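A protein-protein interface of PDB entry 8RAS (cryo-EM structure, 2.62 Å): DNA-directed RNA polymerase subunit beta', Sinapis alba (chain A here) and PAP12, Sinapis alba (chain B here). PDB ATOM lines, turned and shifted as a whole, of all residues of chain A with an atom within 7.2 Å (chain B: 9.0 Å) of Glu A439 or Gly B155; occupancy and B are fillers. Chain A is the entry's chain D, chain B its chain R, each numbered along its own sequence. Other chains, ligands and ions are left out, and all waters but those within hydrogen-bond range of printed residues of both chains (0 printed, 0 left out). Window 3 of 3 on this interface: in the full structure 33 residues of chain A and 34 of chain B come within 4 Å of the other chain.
Of the printed residues of chain B, Trp A438 touches Leu B157. Printed residues of chain A within 4 Å of Gly B120: Glu A443. Printed residues of chain A within 4 Å of Thr B121: Glu A443. Pro B152 touches none of the printed residues of chain A. Printed residues of chain A within 4 Å of Leu B157: Trp A438 and Glu A439. The nearest residue of chain B that does not touch Glu A439 is Pro B154 (4.5 Å). The nearest residue of chain A that does not touch Gly B155 is Pro A435 (5.4 Å). The nearest printed residue of chain B that does not touch Trp A438 is Gly B155 (7.3 Å).
Among the printed residues, no Asp or Glu carboxylate lies within 4 Å of a Lys or Arg side-chain nitrogen of the other chain.
Among the printed residues, pairs that only touch across the chains: Glu A443 with Gly B120 (3.5 Å), Trp A438 with Leu B157 (3.6 Å), Glu A443 with Thr B121 (3.8 Å) and Glu A439 with Leu B157 (3.9 Å).
The backbone NH (N) of Gly B155 lies close to the side-chain carboxylate (OE2) of Glu A439, at 3.3 Å.
NE1 of Trp A438 lies within hydrogen-bond range of O of Lys A434 (3.4 Å).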
ATOM      1  N   GLN A 417     -25.176 -13.921   1.118  1.00  0.00           N
ATOM      2  CA  GLN A 417     -24.510 -15.183   1.415  1.00  0.00           C
ATOM      3  C   GLN A 417     -22.992 -15.069   1.363  1.00  0.00           C
ATOM      4  O   GLN A 417     -22.306 -16.061   1.079  1.00  0.00           O
ATOM      5  CB  GLN A 417     -25.008 -16.278   0.471  1.00  0.00           C
ATOM      6  CG  GLN A 417     -24.795 -15.998  -0.999  1.00  0.00           C
ATOM      7  CD  GLN A 417     -25.413 -17.063  -1.877  1.00  0.00           C
ATOM      8  OE1 GLN A 417     -26.374 -17.724  -1.485  1.00  0.00           O
ATOM      9  NE2 GLN A 417     -24.861 -17.241  -3.071  1.00  0.00           N
ATOM     10  N   LYS A 434     -20.441 -14.900 -14.147  1.00  0.00           N
ATOM     11  CA  LYS A 434     -19.993 -16.034 -13.359  1.00  0.00           C
ATOM     12  C   LYS A 434     -21.120 -17.057 -13.214  1.00  0.00           C
ATOM     13  O   LYS A 434     -22.297 -16.691 -13.157  1.00  0.00           O
ATOM     14  CB  LYS A 434     -19.524 -15.578 -11.980  1.00  0.00           C
ATOM     15  CG  LYS A 434     -18.209 -14.825 -11.995  1.00  0.00           C
ATOM     16  CD  LYS A 434     -17.806 -14.393 -10.596  1.00  0.00           C
ATOM     17  CE  LYS A 434     -16.975 -15.458  -9.901  1.00  0.00           C
ATOM     18  NZ  LYS A 434     -15.595 -15.537 -10.455  1.00  0.00           N
ATOM     19  N   PRO A 435     -20.784 -18.348 -13.157  1.00  0.00           N
ATOM     20  CA  PRO A 435     -21.834 -19.376 -13.064  1.00  0.00           C
ATOM     21  C   PRO A 435     -22.675 -19.282 -11.804  1.00  0.00           C
ATOM     22  O   PRO A 435     -23.799 -19.797 -11.790  1.00  0.00           O
ATOM     23  CB  PRO A 435     -21.045 -20.691 -13.113  1.00  0.00           C
ATOM     24  CG  PRO A 435     -19.660 -20.322 -12.699  1.00  0.00           C
ATOM     25  CD  PRO A 435     -19.439 -18.939 -13.224  1.00  0.00           C
ATOM     26  N   ILE A 436     -22.170 -18.648 -10.743  1.00  0.00           N
ATOM     27  CA  ILE A 436     -22.945 -18.512  -9.512  1.00  0.00           C
ATOM     28  C   ILE A 436     -23.918 -17.345  -9.559  1.00  0.00           C
ATOM     29  O   ILE A 436     -24.816 -17.265  -8.713  1.00  0.00           O
ATOM     30  CB  ILE A 436     -22.007 -18.362  -8.301  1.00  0.00           C
ATOM     31  CG1 ILE A 436     -22.720 -18.787  -7.015  1.00  0.00           C
ATOM     32  CG2 ILE A 436     -21.491 -16.936  -8.201  1.00  0.00           C
ATOM     33  CD1 ILE A 436     -23.340 -20.161  -7.080  1.00  0.00           C
ATOM     34  N   VAL A 437     -23.769 -16.441 -10.527  1.00  0.00           N
ATOM     35  CA  VAL A 437     -24.724 -15.348 -10.674  1.00  0.00           C
ATOM     36  C   VAL A 437     -26.089 -15.889 -11.078  1.00  0.00           C
ATOM     37  O   VAL A 437     -27.129 -15.382 -10.644  1.00  0.00           O
ATOM     38  CB  VAL A 437     -24.195 -14.317 -11.687  1.00  0.00           C
ATOM     39  CG1 VAL A 437     -25.244 -13.260 -11.980  1.00  0.00           C
ATOM     40  CG2 VAL A 437     -22.919 -13.677 -11.168  1.00  0.00           C
ATOM     41  N   TRP A 438     -26.106 -16.939 -11.902  1.00  0.00           N
ATOM     42  CA  TRP A 438     -27.369 -17.468 -12.401  1.00  0.00           C
ATOM     43  C   TRP A 438     -28.133 -18.226 -11.324  1.00  0.00           C
ATOM     44  O   TRP A 438     -29.368 -18.245 -11.346  1.00  0.00           O
ATOM     45  CB  TRP A 438     -27.109 -18.359 -13.612  1.00  0.00           C
ATOM     46  CG  TRP A 438     -26.156 -17.740 -14.581  1.00  0.00           C
ATOM     47  CD1 TRP A 438     -24.930 -18.213 -14.938  1.00  0.00           C
ATOM     48  CD2 TRP A 438     -26.338 -16.514 -15.299  1.00  0.00           C
ATOM     49  NE1 TRP A 438     -24.341 -17.368 -15.844  1.00  0.00           N
ATOM     50  CE2 TRP A 438     -25.187 -16.316 -16.082  1.00  0.00           C
ATOM     51  CE3 TRP A 438     -27.366 -15.570 -15.361  1.00  0.00           C
ATOM     52  CZ2 TRP A 438     -25.033 -15.214 -16.915  1.00  0.00           C
ATOM     53  CZ3 TRP A 438     -27.210 -14.477 -16.186  1.00  0.00           C
ATOM     54  CH2 TRP A 438     -26.056 -14.308 -16.954  1.00  0.00           C
ATOM     55  N   GLU A 439     -27.429 -18.855 -10.383  1.00  0.00           N
ATOM     56  CA  GLU A 439     -28.107 -19.496  -9.261  1.00  0.00           C
ATOM     57  C   GLU A 439     -28.856 -18.470  -8.421  1.00  0.00           C
ATOM     58  O   GLU A 439     -30.018 -18.677  -8.050  1.00  0.00           O
ATOM     59  CB  GLU A 439     -27.098 -20.256  -8.401  1.00  0.00           C
ATOM     60  CG  GLU A 439     -26.884 -21.699  -8.808  1.00  0.00           C
ATOM     61  CD  GLU A 439     -25.908 -22.415  -7.895  1.00  0.00           C
ATOM     62  OE1 GLU A 439     -26.209 -22.551  -6.691  1.00  0.00           O
ATOM     63  OE2 GLU A 439     -24.837 -22.837  -8.380  1.00  0.00           O
ATOM     64  N   ILE A 440     -28.207 -17.344  -8.124  1.00  0.00           N
ATOM     65  CA  ILE A 440     -28.843 -16.308  -7.319  1.00  0.00           C
ATOM     66  C   ILE A 440     -29.986 -15.658  -8.088  1.00  0.00           C
ATOM     67  O   ILE A 440     -31.033 -15.339  -7.514  1.00  0.00           O
ATOM     68  CB  ILE A 440     -27.796 -15.278  -6.859  1.00  0.00           C
ATOM     69  CG1 ILE A 440     -26.924 -15.881  -5.759  1.00  0.00           C
ATOM     70  CG2 ILE A 440     -28.462 -14.009  -6.365  1.00  0.00           C
ATOM     71  CD1 ILE A 440     -25.460 -15.621  -5.935  1.00  0.00           C
ATOM     72  N   LEU A 441     -29.809 -15.453  -9.394  1.00  0.00           N
ATOM     73  CA  LEU A 441     -30.890 -14.902 -10.206  1.00  0.00           C
ATOM     74  C   LEU A 441     -32.098 -15.830 -10.206  1.00  0.00           C
ATOM     75  O   LEU A 441     -33.239 -15.387 -10.030  1.00  0.00           O
ATOM     76  CB  LEU A 441     -30.396 -14.651 -11.631  1.00  0.00           C
ATOM     77  CG  LEU A 441     -31.453 -14.246 -12.659  1.00  0.00           C
ATOM     78  CD1 LEU A 441     -31.979 -12.852 -12.369  1.00  0.00           C
ATOM     79  CD2 LEU A 441     -30.886 -14.324 -14.063  1.00  0.00           C
ATOM     80  N   GLN A 442     -31.859 -17.131 -10.380  1.00  0.00           N
ATOM     81  CA  GLN A 442     -32.949 -18.099 -10.355  1.00  0.00           C
ATOM     82  C   GLN A 442     -33.629 -18.127  -8.993  1.00  0.00           C
ATOM     83  O   GLN A 442     -34.854 -18.273  -8.905  1.00  0.00           O
ATOM     84  CB  GLN A 442     -32.421 -19.485 -10.723  1.00  0.00           C
ATOM     85  CG  GLN A 442     -33.469 -20.423 -11.286  1.00  0.00           C
ATOM     86  CD  GLN A 442     -33.792 -21.565 -10.343  1.00  0.00           C
ATOM     87  OE1 GLN A 442     -32.897 -22.259  -9.861  1.00  0.00           O
ATOM     88  NE2 GLN A 442     -35.077 -21.764 -10.072  1.00  0.00           N
ATOM     89  N   GLU A 443     -32.849 -17.999  -7.918  1.00  0.00           N
ATOM     90  CA  GLU A 443     -33.432 -17.991  -6.581  1.00  0.00           C
ATOM     91  C   GLU A 443     -34.298 -16.758  -6.351  1.00  0.00           C
ATOM     92  O   GLU A 443     -35.410 -16.866  -5.821  1.00  0.00           O
ATOM     93  CB  GLU A 443     -32.327 -18.069  -5.530  1.00  0.00           C
ATOM     94  CG  GLU A 443     -32.807 -18.517  -4.165  1.00  0.00           C
ATOM     95  CD  GLU A 443     -31.692 -18.557  -3.143  1.00  0.00           C
ATOM     96  OE1 GLU A 443     -31.200 -17.476  -2.757  1.00  0.00           O
ATOM     97  OE2 GLU A 443     -31.305 -19.670  -2.727  1.00  0.00           O
ATOM     98  N   VAL A 444     -33.810 -15.579  -6.740  1.00  0.00           N
ATOM     99  CA  VAL A 444     -34.540 -14.349  -6.455  1.00  0.00           C
ATOM    100  C   VAL A 444     -35.712 -14.125  -7.402  1.00  0.00           C
ATOM    101  O   VAL A 444     -36.630 -13.370  -7.061  1.00  0.00           O
ATOM    102  CB  VAL A 444     -33.611 -13.122  -6.487  1.00  0.00           C
ATOM    103  CG1 VAL A 444     -32.449 -13.312  -5.529  1.00  0.00           C
ATOM    104  CG2 VAL A 444     -33.113 -12.859  -7.897  1.00  0.00           C
ATOM    105  N   MET A 445     -35.717 -14.749  -8.581  1.00  0.00           N
ATOM    106  CA  MET A 445     -36.875 -14.615  -9.455  1.00  0.00           C
ATOM    107  C   MET A 445     -38.068 -15.435  -8.984  1.00  0.00           C
ATOM    108  O   MET A 445     -39.186 -15.195  -9.448  1.00  0.00           O
ATOM    109  CB  MET A 445     -36.518 -15.006 -10.889  1.00  0.00           C
ATOM    110  CG  MET A 445     -35.573 -14.039 -11.577  1.00  0.00           C
ATOM    111  SD  MET A 445     -35.485 -14.277 -13.360  1.00  0.00           S
ATOM    112  CE  MET A 445     -36.282 -15.866 -13.538  1.00  0.00           C
ATOM    113  N   GLN A 446     -37.861 -16.387  -8.078  1.00  0.00           N
ATOM    114  CA  GLN A 446     -38.965 -17.187  -7.568  1.00  0.00           C
ATOM    115  C   GLN A 446     -39.875 -16.335  -6.697  1.00  0.00           C
ATOM    116  O   GLN A 446     -39.426 -15.720  -5.726  1.00  0.00           O
ATOM    117  CB  GLN A 446     -38.438 -18.376  -6.767  1.00  0.00           C
ATOM    118  CG  GLN A 446     -37.632 -19.369  -7.575  1.00  0.00           C
ATOM    119  CD  GLN A 446     -37.302 -20.618  -6.784  1.00  0.00           C
ATOM    120  OE1 GLN A 446     -36.145 -21.033  -6.710  1.00  0.00           O
ATOM    121  NE2 GLN A 446     -38.319 -21.223  -6.184  1.00  0.00           N
ATOM    122  N   LEU A 470     -36.450 -18.835 -16.045  1.00  0.00           N
ATOM    123  CA  LEU A 470     -35.288 -18.654 -16.904  1.00  0.00           C
ATOM    124  C   LEU A 470     -35.350 -19.639 -18.065  1.00  0.00           C
ATOM    125  O   LEU A 470     -35.377 -20.855 -17.854  1.00  0.00           O
ATOM    126  CB  LEU A 470     -34.003 -18.843 -16.104  1.00  0.00           C
ATOM    127  CG  LEU A 470     -33.471 -17.598 -15.398  1.00  0.00           C
ATOM    128  CD1 LEU A 470     -32.231 -17.935 -14.590  1.00  0.00           C
ATOM    129  CD2 LEU A 470     -33.182 -16.500 -16.405  1.00  0.00           C
ATOM    130  N   GLY B 120     -35.014 -14.412  -0.765  1.00  0.00           N
ATOM    131  CA  GLY B 120     -34.438 -15.550  -1.449  1.00  0.00           C
ATOM    132  C   GLY B 120     -35.441 -16.662  -1.668  1.00  0.00           C
ATOM    133  O   GLY B 120     -36.394 -16.507  -2.435  1.00  0.00           O
ATOM    134  N   THR B 121     -35.236 -17.795  -0.994  1.00  0.00           N
ATOM    135  CA  THR B 121     -36.184 -18.896  -1.090  1.00  0.00           C
ATOM    136  C   THR B 121     -37.494 -18.590  -0.381  1.00  0.00           C
ATOM    137  O   THR B 121     -38.503 -19.248  -0.657  1.00  0.00           O
ATOM    138  CB  THR B 121     -35.571 -20.173  -0.517  1.00  0.00           C
ATOM    139  OG1 THR B 121     -34.745 -19.842   0.608  1.00  0.00           O
ATOM    140  CG2 THR B 121     -34.728 -20.873  -1.568  1.00  0.00           C
ATOM    141  N   LYS B 151     -31.590 -32.170  -8.183  1.00  0.00           N
ATOM    142  CA  LYS B 151     -30.487 -31.371  -8.698  1.00  0.00           C
ATOM    143  C   LYS B 151     -29.183 -32.142  -8.525  1.00  0.00           C
ATOM    144  O   LYS B 151     -28.874 -32.585  -7.413  1.00  0.00           O
ATOM    145  CB  LYS B 151     -30.413 -30.026  -7.980  1.00  0.00           C
ATOM    146  CG  LYS B 151     -29.883 -28.894  -8.845  1.00  0.00           C
ATOM    147  CD  LYS B 151     -29.594 -27.652  -8.021  1.00  0.00           C
ATOM    148  CE  LYS B 151     -28.486 -27.900  -7.015  1.00  0.00           C
ATOM    149  NZ  LYS B 151     -28.240 -26.710  -6.154  1.00  0.00           N
ATOM    150  N   PRO B 152     -28.398 -32.330  -9.591  1.00  0.00           N
ATOM    151  CA  PRO B 152     -27.210 -33.194  -9.541  1.00  0.00           C
ATOM    152  C   PRO B 152     -25.971 -32.517  -8.959  1.00  0.00           C
ATOM    153  O   PRO B 152     -24.882 -32.577  -9.529  1.00  0.00           O
ATOM    154  CB  PRO B 152     -27.009 -33.572 -11.011  1.00  0.00           C
ATOM    155  CG  PRO B 152     -27.543 -32.415 -11.769  1.00  0.00           C
ATOM    156  CD  PRO B 152     -28.624 -31.777 -10.938  1.00  0.00           C
ATOM    157  N   GLY B 153     -26.137 -31.880  -7.805  1.00  0.00           N
ATOM    158  CA  GLY B 153     -25.036 -31.235  -7.133  1.00  0.00           C
ATOM    159  C   GLY B 153     -24.995 -29.742  -7.383  1.00  0.00           C
ATOM    160  O   GLY B 153     -25.772 -29.198  -8.173  1.00  0.00           O
ATOM    161  N   PRO B 154     -24.077 -29.053  -6.712  1.00  0.00           N
ATOM    162  CA  PRO B 154     -24.012 -27.594  -6.844  1.00  0.00           C
ATOM    163  C   PRO B 154     -23.541 -27.172  -8.225  1.00  0.00           C
ATOM    164  O   PRO B 154     -22.763 -27.864  -8.886  1.00  0.00           O
ATOM    165  CB  PRO B 154     -23.013 -27.171  -5.761  1.00  0.00           C
ATOM    166  CG  PRO B 154     -22.303 -28.411  -5.335  1.00  0.00           C
ATOM    167  CD  PRO B 154     -22.949 -29.610  -5.949  1.00  0.00           C
ATOM    168  N   GLY B 155     -24.030 -26.011  -8.658  1.00  0.00           N
ATOM    169  CA  GLY B 155     -23.671 -25.440  -9.934  1.00  0.00           C
ATOM    170  C   GLY B 155     -24.572 -25.830 -11.085  1.00  0.00           C
ATOM    171  O   GLY B 155     -24.645 -25.090 -12.072  1.00  0.00           O
ATOM    172  N   TYR B 156     -25.274 -26.954 -10.982  1.00  0.00           N
ATOM    173  CA  TYR B 156     -26.125 -27.431 -12.063  1.00  0.00           C
ATOM    174  C   TYR B 156     -27.458 -26.694 -12.030  1.00  0.00           C
ATOM    175  O   TYR B 156     -28.171 -26.731 -11.023  1.00  0.00           O
ATOM    176  CB  TYR B 156     -26.331 -28.938 -11.943  1.00  0.00           C
ATOM    177  CG  TYR B 156     -25.250 -29.756 -12.610  1.00  0.00           C
ATOM    178  CD1 TYR B 156     -24.974 -29.606 -13.961  1.00  0.00           C
ATOM    179  CD2 TYR B 156     -24.490 -30.659 -11.884  1.00  0.00           C
ATOM    180  CE1 TYR B 156     -23.986 -30.350 -14.574  1.00  0.00           C
ATOM    181  CE2 TYR B 156     -23.497 -31.405 -12.488  1.00  0.00           C
ATOM    182  CZ  TYR B 156     -23.249 -31.245 -13.832  1.00  0.00           C
ATOM    183  OH  TYR B 156     -22.260 -31.984 -14.440  1.00  0.00           O
ATOM    184  N   LEU B 157     -27.790 -26.027 -13.130  1.00  0.00           N
ATOM    185  CA  LEU B 157     -29.016 -25.253 -13.249  1.00  0.00           C
ATOM    186  C   LEU B 157     -29.968 -25.964 -14.198  1.00  0.00           C
ATOM    187  O   LEU B 157     -29.571 -26.362 -15.298  1.00  0.00           O
ATOM    188  CB  LEU B 157     -28.724 -23.840 -13.755  1.00  0.00           C
ATOM    189  CG  LEU B 157     -28.081 -22.890 -12.747  1.00  0.00           C
ATOM    190  CD1 LEU B 157     -27.076 -21.986 -13.435  1.00  0.00           C
ATOM    191  CD2 LEU B 157     -29.145 -22.074 -12.036  1.00  0.00           C
ATOM    192  N   LYS B 158     -31.217 -26.123 -13.770  1.00  0.00           N
ATOM    193  CA  LYS B 158     -32.214 -26.778 -14.603  1.00  0.00           C
ATOM    194  C   LYS B 158     -32.497 -25.941 -15.844  1.00  0.00           C
ATOM    195  O   LYS B 158     -32.688 -24.725 -15.757  1.00  0.00           O
ATOM    196  CB  LYS B 158     -33.499 -27.006 -13.809  1.00  0.00           C
ATOM    197  CG  LYS B 158     -34.723 -27.282 -14.665  1.00  0.00           C
ATOM    198  CD  LYS B 158     -35.414 -28.568 -14.245  1.00  0.00           C
ATOM    199  CE  LYS B 158     -36.150 -28.399 -12.927  1.00  0.00           C
ATOM    200  NZ  LYS B 158     -37.076 -27.234 -12.957  1.00  0.00           N
